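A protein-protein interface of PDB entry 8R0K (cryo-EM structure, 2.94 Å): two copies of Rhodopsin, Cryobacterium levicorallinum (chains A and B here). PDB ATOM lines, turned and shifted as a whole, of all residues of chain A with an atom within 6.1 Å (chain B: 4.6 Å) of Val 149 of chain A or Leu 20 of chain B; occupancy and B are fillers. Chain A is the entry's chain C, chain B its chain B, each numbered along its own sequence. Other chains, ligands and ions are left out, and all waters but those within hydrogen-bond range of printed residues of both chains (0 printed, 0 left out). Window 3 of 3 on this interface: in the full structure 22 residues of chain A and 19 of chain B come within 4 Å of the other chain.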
ATOM      1  N   PHE A 141     -16.760   5.783  -6.775  1.00  0.00           N
ATOM      2  CA  PHE A 141     -18.174   6.037  -6.527  1.00  0.00           C
ATOM      3  C   PHE A 141     -18.363   7.462  -6.028  1.00  0.00           C
ATOM      4  O   PHE A 141     -19.303   8.117  -6.460  1.00  0.00           O
ATOM      5  CB  PHE A 141     -18.794   5.072  -5.529  1.00  0.00           C
ATOM      6  CG  PHE A 141     -20.280   5.224  -5.375  1.00  0.00           C
ATOM      7  CD1 PHE A 141     -20.816   5.752  -4.222  1.00  0.00           C
ATOM      8  CD2 PHE A 141     -21.150   4.816  -6.374  1.00  0.00           C
ATOM      9  CE1 PHE A 141     -22.193   5.886  -4.081  1.00  0.00           C
ATOM     10  CE2 PHE A 141     -22.525   4.952  -6.236  1.00  0.00           C
ATOM     11  CZ  PHE A 141     -23.042   5.495  -5.094  1.00  0.00           C
ATOM     12  N   PHE A 144     -18.301   9.661  -8.854  1.00  0.00           N
ATOM     13  CA  PHE A 144     -19.494   9.549  -9.656  1.00  0.00           C
ATOM     14  C   PHE A 144     -20.611  10.389  -9.059  1.00  0.00           C
ATOM     15  O   PHE A 144     -21.389  10.967  -9.809  1.00  0.00           O
ATOM     16  CB  PHE A 144     -19.933   8.096  -9.716  1.00  0.00           C
ATOM     17  CG  PHE A 144     -21.279   7.853 -10.353  1.00  0.00           C
ATOM     18  CD1 PHE A 144     -22.325   7.341  -9.611  1.00  0.00           C
ATOM     19  CD2 PHE A 144     -21.473   8.097 -11.701  1.00  0.00           C
ATOM     20  CE1 PHE A 144     -23.545   7.099 -10.198  1.00  0.00           C
ATOM     21  CE2 PHE A 144     -22.711   7.890 -12.272  1.00  0.00           C
ATOM     22  CZ  PHE A 144     -23.741   7.390 -11.519  1.00  0.00           C
ATOM     23  N   LEU A 145     -20.675  10.461  -7.723  1.00  0.00           N
ATOM     24  CA  LEU A 145     -21.689  11.250  -7.032  1.00  0.00           C
ATOM     25  C   LEU A 145     -21.488  12.731  -7.318  1.00  0.00           C
ATOM     26  O   LEU A 145     -22.434  13.399  -7.748  1.00  0.00           O
ATOM     27  CB  LEU A 145     -21.640  10.996  -5.521  1.00  0.00           C
ATOM     28  CG  LEU A 145     -22.140   9.624  -5.079  1.00  0.00           C
ATOM     29  CD1 LEU A 145     -21.995   9.479  -3.597  1.00  0.00           C
ATOM     30  CD2 LEU A 145     -23.579   9.359  -5.491  1.00  0.00           C
ATOM     31  N   GLY A 146     -20.259  13.209  -7.102  1.00  0.00           N
ATOM     32  CA  GLY A 146     -19.916  14.599  -7.368  1.00  0.00           C
ATOM     33  C   GLY A 146     -20.125  15.041  -8.822  1.00  0.00           C
ATOM     34  O   GLY A 146     -20.726  16.092  -9.085  1.00  0.00           O
ATOM     35  N   ALA A 147     -19.636  14.221  -9.756  1.00  0.00           N
ATOM     36  CA  ALA A 147     -19.580  14.559 -11.165  1.00  0.00           C
ATOM     37  C   ALA A 147     -20.890  14.323 -11.909  1.00  0.00           C
ATOM     38  O   ALA A 147     -21.084  14.971 -12.930  1.00  0.00           O
ATOM     39  CB  ALA A 147     -18.507  13.759 -11.822  1.00  0.00           C
ATOM     40  N   VAL A 148     -21.731  13.377 -11.474  1.00  0.00           N
ATOM     41  CA  VAL A 148     -22.924  13.044 -12.241  1.00  0.00           C
ATOM     42  C   VAL A 148     -24.174  13.137 -11.373  1.00  0.00           C
ATOM     43  O   VAL A 148     -25.130  13.761 -11.809  1.00  0.00           O
ATOM     44  CB  VAL A 148     -22.817  11.662 -12.927  1.00  0.00           C
ATOM     45  CG1 VAL A 148     -24.042  11.333 -13.743  1.00  0.00           C
ATOM     46  CG2 VAL A 148     -21.601  11.557 -13.822  1.00  0.00           C
ATOM     47  N   VAL A 149     -24.208  12.476 -10.204  1.00  0.00           N
ATOM     48  CA  VAL A 149     -25.464  12.272  -9.490  1.00  0.00           C
ATOM     49  C   VAL A 149     -25.866  13.533  -8.732  1.00  0.00           C
ATOM     50  O   VAL A 149     -27.010  13.962  -8.818  1.00  0.00           O
ATOM     51  CB  VAL A 149     -25.429  11.036  -8.571  1.00  0.00           C
ATOM     52  CG1 VAL A 149     -26.594  10.998  -7.600  1.00  0.00           C
ATOM     53  CG2 VAL A 149     -25.430   9.762  -9.389  1.00  0.00           C
ATOM     54  N   ILE A 150     -24.951  14.126  -7.976  1.00  0.00           N
ATOM     55  CA  ILE A 150     -25.359  15.179  -7.051  1.00  0.00           C
ATOM     56  C   ILE A 150     -25.158  16.542  -7.689  1.00  0.00           C
ATOM     57  O   ILE A 150     -24.017  16.976  -7.847  1.00  0.00           O
ATOM     58  CB  ILE A 150     -24.592  15.105  -5.722  1.00  0.00           C
ATOM     59  CG1 ILE A 150     -24.860  13.782  -5.016  1.00  0.00           C
ATOM     60  CG2 ILE A 150     -24.951  16.279  -4.839  1.00  0.00           C
ATOM     61  CD1 ILE A 150     -24.025  13.604  -3.796  1.00  0.00           C
ATOM     62  N   GLY A 151     -26.285  17.217  -7.972  1.00  0.00           N
ATOM     63  CA  GLY A 151     -26.286  18.519  -8.622  1.00  0.00           C
ATOM     64  C   GLY A 151     -26.384  18.415 -10.139  1.00  0.00           C
ATOM     65  O   GLY A 151     -26.361  19.431 -10.827  1.00  0.00           O
ATOM     66  N   ASP A 152     -26.479  17.176 -10.628  1.00  0.00           N
ATOM     67  CA  ASP A 152     -26.637  16.894 -12.043  1.00  0.00           C
ATOM     68  C   ASP A 152     -25.369  17.277 -12.788  1.00  0.00           C
ATOM     69  O   ASP A 152     -25.392  17.449 -14.008  1.00  0.00           O
ATOM     70  CB  ASP A 152     -27.903  17.551 -12.603  1.00  0.00           C
ATOM     71  CG  ASP A 152     -29.188  17.079 -11.924  1.00  0.00           C
ATOM     72  OD1 ASP A 152     -30.273  17.655 -12.229  1.00  0.00           O
ATOM     73  OD2 ASP A 152     -29.109  16.129 -11.093  1.00  0.00           O
ATOM     74  N   GLY A 153     -24.271  17.346 -12.035  1.00  0.00           N
ATOM     75  CA  GLY A 153     -22.980  17.650 -12.613  1.00  0.00           C
ATOM     76  C   GLY A 153     -22.901  19.090 -13.106  1.00  0.00           C
ATOM     77  O   GLY A 153     -22.060  19.385 -13.954  1.00  0.00           O
ATOM     78  N   ALA B  16     -31.183  12.549 -10.549  1.00  0.00           N
ATOM     79  CA  ALA B  16     -30.263  11.848  -9.673  1.00  0.00           C
ATOM     80  C   ALA B  16     -30.667  10.391  -9.550  1.00  0.00           C
ATOM     81  O   ALA B  16     -29.831   9.501  -9.590  1.00  0.00           O
ATOM     82  CB  ALA B  16     -30.249  12.477  -8.307  1.00  0.00           C
ATOM     83  N   GLU B  17     -31.943  10.153  -9.338  1.00  0.00           N
ATOM     84  CA  GLU B  17     -32.374   8.804  -9.111  1.00  0.00           C
ATOM     85  C   GLU B  17     -32.239   8.031 -10.405  1.00  0.00           C
ATOM     86  O   GLU B  17     -31.956   6.845 -10.362  1.00  0.00           O
ATOM     87  CB  GLU B  17     -33.814   8.748  -8.635  1.00  0.00           C
ATOM     88  CG  GLU B  17     -34.024   9.291  -7.243  1.00  0.00           C
ATOM     89  CD  GLU B  17     -35.498   9.476  -6.921  1.00  0.00           C
ATOM     90  OE1 GLU B  17     -35.817   9.821  -5.772  1.00  0.00           O
ATOM     91  OE2 GLU B  17     -36.331   9.307  -7.824  1.00  0.00           O
ATOM     92  N   HIS B  18     -32.420   8.666 -11.546  1.00  0.00           N
ATOM     93  CA  HIS B  18     -32.249   7.945 -12.793  1.00  0.00           C
ATOM     94  C   HIS B  18     -30.782   7.639 -13.033  1.00  0.00           C
ATOM     95  O   HIS B  18     -30.456   6.614 -13.632  1.00  0.00           O
ATOM     96  CB  HIS B  18     -32.749   8.753 -13.959  1.00  0.00           C
ATOM     97  CG  HIS B  18     -32.770   8.094 -15.254  1.00  0.00           C
ATOM     98  ND1 HIS B  18     -31.852   8.440 -16.222  1.00  0.00           N
ATOM     99  CD2 HIS B  18     -33.656   7.274 -15.825  1.00  0.00           C
ATOM    100  CE1 HIS B  18     -32.182   7.832 -17.356  1.00  0.00           C
ATOM    101  NE2 HIS B  18     -33.274   7.094 -17.127  1.00  0.00           N
ATOM    102  N   SER B  19     -29.893   8.490 -12.517  1.00  0.00           N
ATOM    103  CA  SER B  19     -28.466   8.206 -12.596  1.00  0.00           C
ATOM    104  C   SER B  19     -28.092   7.059 -11.661  1.00  0.00           C
ATOM    105  O   SER B  19     -27.514   6.071 -12.094  1.00  0.00           O
ATOM    106  CB  SER B  19     -27.645   9.439 -12.351  1.00  0.00           C
ATOM    107  OG  SER B  19     -27.922  10.395 -13.370  1.00  0.00           O
ATOM    108  N   LEU B  20     -28.438   7.167 -10.392  1.00  0.00           N
ATOM    109  CA  LEU B  20     -28.087   6.091  -9.505  1.00  0.00           C
ATOM    110  C   LEU B  20     -28.613   4.793 -10.091  1.00  0.00           C
ATOM    111  O   LEU B  20     -27.867   3.834 -10.186  1.00  0.00           O
ATOM    112  CB  LEU B  20     -28.660   6.352  -8.116  1.00  0.00           C
ATOM    113  CG  LEU B  20     -27.936   7.445  -7.335  1.00  0.00           C
ATOM    114  CD1 LEU B  20     -28.658   7.781  -6.043  1.00  0.00           C
ATOM    115  CD2 LEU B  20     -26.494   7.046  -7.038  1.00  0.00           C
ATOM    116  N   ILE B  21     -29.876   4.752 -10.499  1.00  0.00           N
ATOM    117  CA  ILE B  21     -30.485   3.483 -10.854  1.00  0.00           C
ATOM    118  C   ILE B  21     -29.781   2.861 -12.040  1.00  0.00           C
ATOM    119  O   ILE B  21     -29.721   1.639 -12.099  1.00  0.00           O
ATOM    120  CB  ILE B  21     -31.987   3.590 -11.135  1.00  0.00           C
ATOM    121  CG1 ILE B  21     -32.714   3.999  -9.859  1.00  0.00           C
ATOM    122  CG2 ILE B  21     -32.520   2.278 -11.673  1.00  0.00           C
ATOM    123  CD1 ILE B  21     -34.203   4.058 -10.021  1.00  0.00           C
ATOM    124  N   PHE B  22     -29.255   3.678 -12.953  1.00  0.00           N
ATOM    125  CA  PHE B  22     -28.483   3.152 -14.070  1.00  0.00           C
ATOM    126  C   PHE B  22     -27.136   2.605 -13.610  1.00  0.00           C
ATOM    127  O   PHE B  22     -26.770   1.496 -13.962  1.00  0.00           O
ATOM    128  CB  PHE B  22     -28.224   4.219 -15.127  1.00  0.00           C
ATOM    129  CG  PHE B  22     -27.246   3.802 -16.196  1.00  0.00           C
ATOM    130  CD1 PHE B  22     -25.882   4.051 -16.058  1.00  0.00           C
ATOM    131  CD2 PHE B  22     -27.680   3.176 -17.364  1.00  0.00           C
ATOM    132  CE1 PHE B  22     -24.987   3.670 -17.055  1.00  0.00           C
ATOM    133  CE2 PHE B  22     -26.780   2.796 -18.361  1.00  0.00           C
ATOM    134  CZ  PHE B  22     -25.435   3.050 -18.205  1.00  0.00           C
ATOM    135  N   TYR B  23     -26.400   3.363 -12.811  1.00  0.00           N
ATOM    136  CA  TYR B  23     -25.089   2.939 -12.376  1.00  0.00           C
ATOM    137  C   TYR B  23     -25.145   1.562 -11.748  1.00  0.00           C
ATOM    138  O   TYR B  23     -24.279   0.752 -12.029  1.00  0.00           O
ATOM    139  CB  TYR B  23     -24.566   3.920 -11.344  1.00  0.00           C
ATOM    140  CG  TYR B  23     -23.250   3.556 -10.690  1.00  0.00           C
ATOM    141  CD1 TYR B  23     -23.222   2.874  -9.484  1.00  0.00           C
ATOM    142  CD2 TYR B  23     -22.043   3.969 -11.239  1.00  0.00           C
ATOM    143  CE1 TYR B  23     -22.020   2.579  -8.871  1.00  0.00           C
ATOM    144  CE2 TYR B  23     -20.838   3.682 -10.636  1.00  0.00           C
ATOM    145  CZ  TYR B  23     -20.833   2.978  -9.454  1.00  0.00           C
ATOM    146  OH  TYR B  23     -19.676   2.636  -8.836  1.00  0.00           O
ATOM    147  N   PHE B  24     -26.119   1.304 -10.872  1.00  0.00           N
ATOM    148  CA  PHE B  24     -26.184   0.026 -10.191  1.00  0.00           C
ATOM    149  C   PHE B  24     -26.661  -1.062 -11.145  1.00  0.00           C
ATOM    150  O   PHE B  24     -26.239  -2.210 -11.016  1.00  0.00           O
ATOM    151  CB  PHE B  24     -27.032   0.115  -8.947  1.00  0.00           C
ATOM    152  CG  PHE B  24     -26.352   0.879  -7.856  1.00  0.00           C
ATOM    153  CD1 PHE B  24     -25.455   0.284  -6.999  1.00  0.00           C
ATOM    154  CD2 PHE B  24     -26.663   2.200  -7.634  1.00  0.00           C
ATOM    155  CE1 PHE B  24     -24.891   0.993  -5.947  1.00  0.00           C
ATOM    156  CE2 PHE B  24     -26.095   2.909  -6.581  1.00  0.00           C
ATOM    157  CZ  PHE B  24     -25.190   2.308  -5.751  1.00  0.00           C
ATOM    158  N   THR B 227     -35.516   3.753  -6.363  1.00  0.00           N
ATOM    159  CA  THR B 227     -34.075   3.769  -6.304  1.00  0.00           C
ATOM    160  C   THR B 227     -33.559   2.833  -5.219  1.00  0.00           C
ATOM    161  O   THR B 227     -32.636   2.079  -5.461  1.00  0.00           O
ATOM    162  CB  THR B 227     -33.584   5.199  -6.091  1.00  0.00           C
ATOM    163  OG1 THR B 227     -34.256   5.964  -7.093  1.00  0.00           O
ATOM    164  CG2 THR B 227     -32.084   5.359  -6.216  1.00  0.00           C
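No position is printed for both chains.
Among the printed residues, merely in contact across the chains: Phe 141 of chain A with Tyr 23 of chain B (3.5 Å), Phe 144 of chain A with Tyr 23 of chain B (3.5 Å), Val 149 of chain A with Ala 16 of chain B (3.6 Å), Val 149 of chain A with Ser 19 of chain B (3.7 Å), Val 149 of chain A with Leu 20 of chain B (3.7 Å) and Phe 141 of chain A with Phe 24 of chain B (3.8 Å).
The backbone carbonyl oxygen of Phe 144 of chain A lies within hydrogen-bond range of the backbone NH of Val 149 of chain A (3.2 Å).
Hydrophobic or aromatic side chains of chain B that line the printed part of chain A: Ala 16, Leu 20, Tyr 23 and Phe 24. Among the printed residues, 6 pairs touch across the chains.
Of the printed residues of chain B, Phe 141 of chain A touches Tyr 23 (3.5 Å) and Phe 24 (3.8 Å). Of chain B, only Ala 16, Ser 19 and Leu 20 come within 4 Å of Val 149 of chain A. Leu 20 of chain B touches just one residue of chain A: Val 149 (3.7 Å). Printed residues of chain A within 4 Å of Tyr 23 of chain B: Phe 141 (3.5 Å) and Phe 144 (3.5 Å). Of the printed residues of chain A, Phe 24 of chain B touches Phe 141 (3.8 Å). The nearest printed residue of chain B that does not touch Val 149 of chain A is Glu 17 of chain B (5.7 Å).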
